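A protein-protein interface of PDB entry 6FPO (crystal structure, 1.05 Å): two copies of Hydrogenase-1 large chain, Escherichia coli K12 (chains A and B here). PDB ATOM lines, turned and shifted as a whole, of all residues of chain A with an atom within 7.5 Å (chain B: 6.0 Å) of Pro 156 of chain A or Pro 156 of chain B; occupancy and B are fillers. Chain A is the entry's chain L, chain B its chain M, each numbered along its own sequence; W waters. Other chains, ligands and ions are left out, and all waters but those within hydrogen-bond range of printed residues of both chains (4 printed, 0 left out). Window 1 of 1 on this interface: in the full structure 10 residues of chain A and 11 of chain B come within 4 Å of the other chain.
The side-chain amide oxygen of Gln 150 of chain B is in hydrogen-bond range of the side-chain amide nitrogen of Gln 150 of chain A (2.9 Å).
OG of Ser 159 of chain B lies within hydrogen-bond range of O of Ser 154 of chain A, at 3.0 Å.
The backbone carbonyl oxygen (O) of Trp 155 of chain A sits at hydrogen-bond distance from the side-chain hydroxyl (OG) of Ser 159 of chain B, at 3.1 Å.
The backbone carbonyl oxygen of Pro 156 of chain A is in hydrogen-bond range of the backbone NH of Ser 158 of chain B, at 3.0 Å.
O of Pro 156 of chain A is in hydrogen-bond range of N of Ser 159 of chain B (3.2 Å).
O of Pro 156 of chain B lies within hydrogen-bond range of N of Ser 158 of chain A, 3.1 Å away.
OG of Ser 159 of chain A is in hydrogen-bond range of O of Ser 154 of chain B (3.0 Å).
The side-chain hydroxyl (OG) of Ser 159 of chain A is in hydrogen-bond range of the backbone carbonyl oxygen (O) of Trp 155 of chain B (3.1 Å).
The backbone NH of Ser 159 of chain A lies within hydrogen-bond range of the backbone carbonyl oxygen of Pro 156 of chain B (3.3 Å).
The backbone NH (N) of Tyr 162 of chain A lies within hydrogen-bond range of the backbone carbonyl oxygen (O) of Ser 154 of chain B (3.5 Å).
The backbone carbonyl oxygen (O) of Pro 156 of chain A sits close to the backbone carbonyl oxygen (O) of Pro 156 of chain B.
NE2 of Gln 150 of chain A lies within hydrogen-bond range of OG of Ser 158 of chain A.
N of Trp 155 of chain A sits at hydrogen-bond distance from OG of Ser 153 of chain A (2.9 Å).
OG of Ser 154 of chain A is in hydrogen-bond range of OD1 of Asn 273 of chain A (3.3 Å).
N of Tyr 162 of chain A sits at hydrogen-bond distance from OG of Ser 159 of chain A, at 2.9 Å.
The side-chain hydroxyl (OH) of Tyr 162 of chain A sits at hydrogen-bond distance from the side-chain carboxylate (OE1) of Glu 208 of chain A (2.5 Å).
The side-chain hydroxyl of Ser 159 of chain B is in hydrogen-bond range of the backbone NH of Tyr 162 of chain B, at 2.9 Å.
Among the printed residues, merely in contact across the chains: Ser 158 of chain A with Ser 159 of chain B (3.2 Å), Ser 159 of chain A with Ser 158 of chain B (3.2 Å), Pro 156 of chain A with Lys 157 of chain B (3.4 Å), Lys 157 of chain A with Pro 156 of chain B (3.4 Å), Pro 160 of chain A with Gln 150 of chain B (3.4 Å), Ser 154 of chain A with Tyr 162 of chain B (3.5 Å), Tyr 162 of chain A with Pro 156 of chain B (3.6 Å), Pro 156 of chain A with Tyr 162 of chain B (3.6 Å), Ser 159 of chain A with Gln 150 of chain B (3.7 Å), Gln 150 of chain A with Ser 159 of chain B (3.8 Å), Gly 161 of chain A with Ser 154 of chain B (3.9 Å) and Lys 157 of chain A with Lys 157 of chain B (3.9 Å).
Of chain B, only Pro 156 (3.1 Å), Lys 157 (3.4 Å), Ser 158 (3.0 Å), Ser 159 (3.2 Å) and Tyr 162 (3.6 Å) come within 4 Å of Pro 156 of chain A.
Printed residues of chain B within 4 Å of Tyr 162 of chain A: Ser 154 and Pro 156.
Of the printed residues of chain A, Trp 155 of chain B touches Ser 159.
Asn 273 of chain A touches none of the printed residues of chain B.
Glu 208 of chain A touches none of the printed residues of chain B.
The nearest printed residue of chain B that does not touch Pro 156 of chain A is Trp 155 of chain B (6.3 Å).
The nearest printed residue of chain A that does not touch Gln 150 of chain B is Ser 158 of chain A (4.2 Å).
Hydrophobic or aromatic side chains of chain A that line the printed part of chain B: Pro 156, Pro 160 and Tyr 162.
Among the printed residues, 23 pairs touch across the chains.
Among the printed residues, no Asp or Glu carboxylate lies within 4 Å of a Lys or Arg side-chain nitrogen of the other chain.
Gln 150 of chain A touches Ser 159 of chain B, and with the chains exchanged Ser 159 of chain A touches Gln 150 of chain B.
Ser 154 of chain A touches Tyr 162 of chain B, and with the chains exchanged Tyr 162 of chain A touches Ser 154 of chain B.
Trp 155 of chain A touches Ser 159 of chain B, and with the chains exchanged Ser 159 of chain A touches Trp 155 of chain B.
Ser 158 of chain A touches Ser 159 of chain B, and with the chains exchanged Ser 159 of chain A touches Ser 158 of chain B.
Positions printed for both chains: 150, 154, 155, 156, 157, 158, 159 and 162.
Of the 23 pairs that touch across the chains among the printed residues, 21 have their exchanged pair printed and touching as well.
Water W4 bridges the side-chain carboxylate of Asp 165 of chain A (2.6 Å) and the backbone carbonyl oxygen of Ser 154 of chain B (2.9 Å).
Water W1 bridges the backbone NH of Gly 161 of chain A (3.0 Å) and the backbone carbonyl oxygen of Gln 150 of chain B (3.5 Å).
Water W3 lies within hydrogen-bond range of the side-chain amide oxygen (OE1) of Gln 150 of chain A (3.0 Å) and the side-chain amide nitrogen (NE2) of Gln 150 of chain B (3.2 Å).
Water W2 bridges the side-chain amide nitrogen of Gln 150 of chain B and the side-chain amide oxygen of Gln 150 of chain A.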
ATOM      1  N   GLN A 150      13.810  20.316  12.362  1.00  0.00           N
ATOM      2  CA  GLN A 150      14.463  19.913  11.142  1.00  0.00           C
ATOM      3  C   GLN A 150      15.906  19.561  11.354  1.00  0.00           C
ATOM      4  O   GLN A 150      16.456  18.749  10.596  1.00  0.00           O
ATOM      5  CB  GLN A 150      14.259  21.005  10.086  1.00  0.00           C
ATOM      6  CG  GLN A 150      12.816  21.122   9.688  1.00  0.00           C
ATOM      7  CD  GLN A 150      12.460  22.230   8.730  1.00  0.00           C
ATOM      8  OE1 GLN A 150      13.310  23.031   8.306  1.00  0.00           O
ATOM      9  NE2 GLN A 150      11.268  22.256   8.317  1.00  0.00           N
ATOM     10  N   SER A 153      15.667  15.732  12.844  1.00  0.00           N
ATOM     11  CA  SER A 153      14.955  14.614  12.218  1.00  0.00           C
ATOM     12  C   SER A 153      14.543  14.953  10.810  1.00  0.00           C
ATOM     13  O   SER A 153      14.254  16.131  10.466  1.00  0.00           O
ATOM     14  CB  SER A 153      13.692  14.291  13.045  1.00  0.00           C
ATOM     15  OG  SER A 153      12.975  13.217  12.443  1.00  0.00           O
ATOM     16  N   SER A 154      14.364  13.883  10.044  1.00  0.00           N
ATOM     17  CA  SER A 154      13.727  13.985   8.732  1.00  0.00           C
ATOM     18  C   SER A 154      12.217  14.008   8.781  1.00  0.00           C
ATOM     19  O   SER A 154      11.554  14.122   7.737  1.00  0.00           O
ATOM     20  CB  SER A 154      14.188  12.824   7.885  1.00  0.00           C
ATOM     21  OG  SER A 154      13.896  11.581   8.506  1.00  0.00           O
ATOM     22  N   TRP A 155      11.625  13.823   9.960  1.00  0.00           N
ATOM     23  CA  TRP A 155      10.161  13.706  10.104  1.00  0.00           C
ATOM     24  C   TRP A 155       9.484  14.828   9.296  1.00  0.00           C
ATOM     25  O   TRP A 155       9.890  15.979   9.363  1.00  0.00           O
ATOM     26  CB  TRP A 155       9.748  13.827  11.550  1.00  0.00           C
ATOM     27  CG  TRP A 155       8.295  13.583  11.836  1.00  0.00           C
ATOM     28  CD1 TRP A 155       7.459  14.438  12.499  1.00  0.00           C
ATOM     29  CD2 TRP A 155       7.574  12.380  11.591  1.00  0.00           C
ATOM     30  NE1 TRP A 155       6.225  13.820  12.639  1.00  0.00           N
ATOM     31  CE2 TRP A 155       6.291  12.555  12.102  1.00  0.00           C
ATOM     32  CE3 TRP A 155       7.901  11.148  11.011  1.00  0.00           C
ATOM     33  CZ2 TRP A 155       5.318  11.505  12.043  1.00  0.00           C
ATOM     34  CZ3 TRP A 155       6.999  10.156  10.969  1.00  0.00           C
ATOM     35  CH2 TRP A 155       5.740  10.337  11.475  1.00  0.00           C
ATOM     36  N   PRO A 156       8.451  14.502   8.505  1.00  0.00           N
ATOM     37  CA  PRO A 156       7.908  15.594   7.637  1.00  0.00           C
ATOM     38  C   PRO A 156       7.287  16.762   8.354  1.00  0.00           C
ATOM     39  O   PRO A 156       7.352  17.850   7.823  1.00  0.00           O
ATOM     40  CB  PRO A 156       6.885  14.839   6.790  1.00  0.00           C
ATOM     41  CG  PRO A 156       7.433  13.406   6.711  1.00  0.00           C
ATOM     42  CD  PRO A 156       7.953  13.197   8.107  1.00  0.00           C
ATOM     43  N   LYS A 157       6.635  16.529   9.494  1.00  0.00           N
ATOM     44  CA  LYS A 157       5.735  17.507  10.077  1.00  0.00           C
ATOM     45  C   LYS A 157       6.542  18.493  10.916  1.00  0.00           C
ATOM     46  O   LYS A 157       6.720  18.315  12.100  1.00  0.00           O
ATOM     47  CB  LYS A 157       4.676  16.816  10.910  1.00  0.00           C
ATOM     48  CG  LYS A 157       3.803  15.917  10.078  1.00  0.00           C
ATOM     49  CD  LYS A 157       2.634  15.391  10.949  1.00  0.00           C
ATOM     50  CE  LYS A 157       1.757  14.530  10.146  1.00  0.00           C
ATOM     51  NZ  LYS A 157       0.711  13.979  11.007  1.00  0.00           N
ATOM     52  N   SER A 158       6.987  19.560  10.250  1.00  0.00           N
ATOM     53  CA  SER A 158       7.932  20.485  10.851  1.00  0.00           C
ATOM     54  C   SER A 158       7.729  21.906  10.420  1.00  0.00           C
ATOM     55  O   SER A 158       8.586  22.734  10.734  1.00  0.00           O
ATOM     56  CB  SER A 158       9.399  20.058  10.495  1.00  0.00           C
ATOM     57  OG  SER A 158       9.545  20.248   9.102  1.00  0.00           O
ATOM     58  N   SER A 159       6.673  22.242   9.682  1.00  0.00           N
ATOM     59  CA  SER A 159       6.608  23.597   9.163  1.00  0.00           C
ATOM     60  C   SER A 159       6.407  24.612  10.293  1.00  0.00           C
ATOM     61  O   SER A 159       5.789  24.320  11.309  1.00  0.00           O
ATOM     62  CB  SER A 159       5.463  23.738   8.161  1.00  0.00           C
ATOM     63  OG  SER A 159       4.212  23.736   8.806  1.00  0.00           O
ATOM     64  N   PRO A 160       6.868  25.876  10.070  1.00  0.00           N
ATOM     65  CA  PRO A 160       6.576  26.914  11.015  1.00  0.00           C
ATOM     66  C   PRO A 160       5.062  27.076  11.243  1.00  0.00           C
ATOM     67  O   PRO A 160       4.607  27.318  12.373  1.00  0.00           O
ATOM     68  CB  PRO A 160       7.171  28.162  10.360  1.00  0.00           C
ATOM     69  CG  PRO A 160       8.266  27.618   9.523  1.00  0.00           C
ATOM     70  CD  PRO A 160       7.755  26.320   8.984  1.00  0.00           C
ATOM     71  N   GLY A 161       4.272  26.959  10.162  1.00  0.00           N
ATOM     72  CA  GLY A 161       2.842  27.119  10.298  1.00  0.00           C
ATOM     73  C   GLY A 161       2.220  26.034  11.166  1.00  0.00           C
ATOM     74  O   GLY A 161       1.267  26.285  11.912  1.00  0.00           O
ATOM     75  N   TYR A 162       2.722  24.815  11.054  1.00  0.00           N
ATOM     76  CA  TYR A 162       2.280  23.739  11.936  1.00  0.00           C
ATOM     77  C   TYR A 162       2.566  24.032  13.389  1.00  0.00           C
ATOM     78  O   TYR A 162       1.686  23.899  14.233  1.00  0.00           O
ATOM     79  CB  TYR A 162       2.994  22.445  11.520  1.00  0.00           C
ATOM     80  CG  TYR A 162       2.813  21.272  12.446  1.00  0.00           C
ATOM     81  CD1 TYR A 162       1.532  20.791  12.756  1.00  0.00           C
ATOM     82  CD2 TYR A 162       3.894  20.628  12.984  1.00  0.00           C
ATOM     83  CE1 TYR A 162       1.384  19.712  13.597  1.00  0.00           C
ATOM     84  CE2 TYR A 162       3.760  19.510  13.800  1.00  0.00           C
ATOM     85  CZ  TYR A 162       2.520  19.074  14.127  1.00  0.00           C
ATOM     86  OH  TYR A 162       2.350  17.989  14.964  1.00  0.00           O
ATOM     87  N   PHE A 163       3.796  24.450  13.704  1.00  0.00           N
ATOM     88  CA  PHE A 163       4.101  24.753  15.101  1.00  0.00           C
ATOM     89  C   PHE A 163       3.281  25.933  15.597  1.00  0.00           C
ATOM     90  O   PHE A 163       2.860  25.936  16.761  1.00  0.00           O
ATOM     91  CB  PHE A 163       5.626  24.900  15.284  1.00  0.00           C
ATOM     92  CG  PHE A 163       6.340  23.586  15.164  1.00  0.00           C
ATOM     93  CD1 PHE A 163       6.043  22.525  16.024  1.00  0.00           C
ATOM     94  CD2 PHE A 163       7.305  23.370  14.192  1.00  0.00           C
ATOM     95  CE1 PHE A 163       6.695  21.312  15.931  1.00  0.00           C
ATOM     96  CE2 PHE A 163       7.984  22.179  14.110  1.00  0.00           C
ATOM     97  CZ  PHE A 163       7.656  21.118  14.966  1.00  0.00           C
ATOM     98  N   ASP A 165       0.281  26.667  14.559  1.00  0.00           N
ATOM     99  CA  ASP A 165      -1.081  26.103  14.723  1.00  0.00           C
ATOM    100  C   ASP A 165      -1.188  25.322  16.045  1.00  0.00           C
ATOM    101  O   ASP A 165      -2.146  25.481  16.804  1.00  0.00           O
ATOM    102  CB  ASP A 165      -1.501  25.208  13.540  1.00  0.00           C
ATOM    103  CG  ASP A 165      -1.795  26.003  12.242  1.00  0.00           C
ATOM    104  OD1 ASP A 165      -1.967  27.214  12.311  1.00  0.00           O
ATOM    105  OD2 ASP A 165      -1.912  25.342  11.192  1.00  0.00           O
ATOM    106  N   GLU A 208       0.921  14.246  18.474  1.00  0.00           N
ATOM    107  CA  GLU A 208       1.064  13.291  17.384  1.00  0.00           C
ATOM    108  C   GLU A 208       1.103  11.866  17.894  1.00  0.00           C
ATOM    109  O   GLU A 208       0.528  10.956  17.253  1.00  0.00           O
ATOM    110  CB  GLU A 208       2.319  13.557  16.552  1.00  0.00           C
ATOM    111  CG  GLU A 208       2.263  14.836  15.745  1.00  0.00           C
ATOM    112  CD  GLU A 208       3.452  15.012  14.855  1.00  0.00           C
ATOM    113  OE1 GLU A 208       4.009  16.149  14.845  1.00  0.00           O
ATOM    114  OE2 GLU A 208       3.849  14.082  14.134  1.00  0.00           O
ATOM    115  N   ASP A 269       8.369   3.931  11.392  1.00  0.00           N
ATOM    116  CA  ASP A 269       8.685   5.293  10.975  1.00  0.00           C
ATOM    117  C   ASP A 269       8.438   6.314  12.083  1.00  0.00           C
ATOM    118  O   ASP A 269       9.257   7.199  12.293  1.00  0.00           O
ATOM    119  CB  ASP A 269       7.950   5.659   9.703  1.00  0.00           C
ATOM    120  CG  ASP A 269       8.481   4.924   8.497  1.00  0.00           C
ATOM    121  OD1 ASP A 269       9.501   4.270   8.616  1.00  0.00           O
ATOM    122  OD2 ASP A 269       7.851   4.942   7.483  1.00  0.00           O
ATOM    123  N   ASN A 273      11.629   8.309  13.814  1.00  0.00           N
ATOM    124  CA  ASN A 273      11.762   9.704  13.426  1.00  0.00           C
ATOM    125  C   ASN A 273      11.123  10.700  14.336  1.00  0.00           C
ATOM    126  O   ASN A 273      11.360  11.911  14.147  1.00  0.00           O
ATOM    127  CB  ASN A 273      11.284   9.854  11.977  1.00  0.00           C
ATOM    128  CG  ASN A 273      12.151   9.014  11.030  1.00  0.00           C
ATOM    129  OD1 ASN A 273      13.309   9.300  10.865  1.00  0.00           O
ATOM    130  ND2 ASN A 273      11.593   7.961  10.492  1.00  0.00           N
ATOM    131  N   VAL A 274      10.369  10.249  15.341  1.00  0.00           N
ATOM    132  CA  VAL A 274       9.753  11.130  16.320  1.00  0.00           C
ATOM    133  C   VAL A 274      10.312  10.802  17.711  1.00  0.00           C
ATOM    134  O   VAL A 274      10.963  11.614  18.343  1.00  0.00           O
ATOM    135  CB  VAL A 274       8.202  11.105  16.261  1.00  0.00           C
ATOM    136  CG1 VAL A 274       7.635  12.136  17.209  1.00  0.00           C
ATOM    137  CG2 VAL A 274       7.731  11.350  14.845  1.00  0.00           C
ATOM    138  N   GLN B 150       7.057  26.072   2.651  1.00  0.00           N
ATOM    139  CA  GLN B 150       6.727  26.825   3.880  1.00  0.00           C
ATOM    140  C   GLN B 150       6.339  28.258   3.628  1.00  0.00           C
ATOM    141  O   GLN B 150       5.565  28.827   4.388  1.00  0.00           O
ATOM    142  CB  GLN B 150       7.872  26.699   4.870  1.00  0.00           C
ATOM    143  CG  GLN B 150       8.078  25.251   5.318  1.00  0.00           C
ATOM    144  CD  GLN B 150       9.223  24.924   6.231  1.00  0.00           C
ATOM    145  OE1 GLN B 150       9.344  23.784   6.730  1.00  0.00           O
ATOM    146  NE2 GLN B 150      10.064  25.823   6.458  1.00  0.00           N
ATOM    147  N   SER B 154       0.875  26.661   5.470  1.00  0.00           N
ATOM    148  CA  SER B 154       1.063  26.137   6.804  1.00  0.00           C
ATOM    149  C   SER B 154       1.090  24.614   6.869  1.00  0.00           C
ATOM    150  O   SER B 154       1.345  24.062   7.948  1.00  0.00           O
ATOM    151  CB  SER B 154      -0.037  26.667   7.734  1.00  0.00           C
ATOM    152  OG  SER B 154      -1.300  26.302   7.200  1.00  0.00           O
ATOM    153  N   TRP B 155       0.861  23.931   5.744  1.00  0.00           N
ATOM    154  CA  TRP B 155       0.764  22.465   5.746  1.00  0.00           C
ATOM    155  C   TRP B 155       1.959  21.890   6.493  1.00  0.00           C
ATOM    156  O   TRP B 155       3.094  22.282   6.296  1.00  0.00           O
ATOM    157  CB  TRP B 155       0.804  21.938   4.308  1.00  0.00           C
ATOM    158  CG  TRP B 155       0.592  20.494   4.152  1.00  0.00           C
ATOM    159  CD1 TRP B 155       1.425  19.616   3.503  1.00  0.00           C
ATOM    160  CD2 TRP B 155      -0.564  19.746   4.551  1.00  0.00           C
ATOM    161  NE1 TRP B 155       0.820  18.378   3.491  1.00  0.00           N
ATOM    162  CE2 TRP B 155      -0.397  18.450   4.109  1.00  0.00           C
ATOM    163  CE3 TRP B 155      -1.762  20.076   5.200  1.00  0.00           C
ATOM    164  CZ2 TRP B 155      -1.396  17.457   4.286  1.00  0.00           C
ATOM    165  CZ3 TRP B 155      -2.755  19.097   5.379  1.00  0.00           C
ATOM    166  CH2 TRP B 155      -2.547  17.836   4.961  1.00  0.00           C
ATOM    167  N   PRO B 156       1.745  20.909   7.387  1.00  0.00           N
ATOM    168  CA  PRO B 156       2.892  20.461   8.202  1.00  0.00           C
ATOM    169  C   PRO B 156       4.013  19.827   7.444  1.00  0.00           C
ATOM    170  O   PRO B 156       5.154  19.980   7.826  1.00  0.00           O
ATOM    171  CB  PRO B 156       2.247  19.529   9.214  1.00  0.00           C
ATOM    172  CG  PRO B 156       0.827  20.023   9.330  1.00  0.00           C
ATOM    173  CD  PRO B 156       0.464  20.419   7.951  1.00  0.00           C
ATOM    174  N   LYS B 157       3.682  19.020   6.436  1.00  0.00           N
ATOM    175  CA  LYS B 157       4.638  18.106   5.822  1.00  0.00           C
ATOM    176  C   LYS B 157       5.517  18.836   4.824  1.00  0.00           C
ATOM    177  O   LYS B 157       5.226  18.935   3.637  1.00  0.00           O
ATOM    178  CB  LYS B 157       3.926  16.907   5.142  1.00  0.00           C
ATOM    179  CG  LYS B 157       3.163  16.037   6.130  1.00  0.00           C
ATOM    180  CD  LYS B 157       2.513  14.891   5.415  1.00  0.00           C
ATOM    181  CE  LYS B 157       1.710  14.026   6.253  1.00  0.00           C
ATOM    182  NZ  LYS B 157       1.305  12.866   5.415  1.00  0.00           N
ATOM    183  N   SER B 158       6.634  19.377   5.338  1.00  0.00           N
ATOM    184  CA  SER B 158       7.463  20.266   4.549  1.00  0.00           C
ATOM    185  C   SER B 158       8.921  20.194   4.908  1.00  0.00           C
ATOM    186  O   SER B 158       9.675  21.022   4.422  1.00  0.00           O
ATOM    187  CB  SER B 158       7.005  21.720   4.786  1.00  0.00           C
ATOM    188  OG  SER B 158       7.255  22.000   6.175  1.00  0.00           O
ATOM    189  N   SER B 159       9.366  19.237   5.703  1.00  0.00           N
ATOM    190  CA  SER B 159      10.762  19.233   6.115  1.00  0.00           C
ATOM    191  C   SER B 159      11.709  18.981   4.939  1.00  0.00           C
ATOM    192  O   SER B 159      11.362  18.294   4.005  1.00  0.00           O
ATOM    193  CB  SER B 159      11.045  18.210   7.219  1.00  0.00           C
ATOM    194  OG  SER B 159      11.052  16.896   6.658  1.00  0.00           O
ATOM    195  N   TYR B 162      11.912  15.272   4.442  1.00  0.00           N
ATOM    196  CA  TYR B 162      10.762  14.725   3.679  1.00  0.00           C
ATOM    197  C   TYR B 162      10.972  14.875   2.200  1.00  0.00           C
ATOM    198  O   TYR B 162      10.793  13.936   1.434  1.00  0.00           O
ATOM    199  CB  TYR B 162       9.500  15.450   4.152  1.00  0.00           C
ATOM    200  CG  TYR B 162       8.277  15.200   3.325  1.00  0.00           C
ATOM    201  CD1 TYR B 162       7.768  13.932   3.162  1.00  0.00           C
ATOM    202  CD2 TYR B 162       7.616  16.201   2.718  1.00  0.00           C
ATOM    203  CE1 TYR B 162       6.612  13.703   2.422  1.00  0.00           C
ATOM    204  CE2 TYR B 162       6.470  15.985   1.965  1.00  0.00           C
ATOM    205  CZ  TYR B 162       5.957  14.734   1.844  1.00  0.00           C
ATOM    206  OH  TYR B 162       4.840  14.532   1.085  1.00  0.00           O
HETATM  207  O   HOH W   1       4.754  27.002   7.248  1.00  0.00           O
HETATM  208  O   HOH W   2      12.039  26.097   8.742  1.00  0.00           O
HETATM  209  O   HOH W   3      13.029  24.755   5.912  1.00  0.00           O
HETATM  210  O   HOH W   4      -0.589  23.354  10.048  1.00  0.00           O
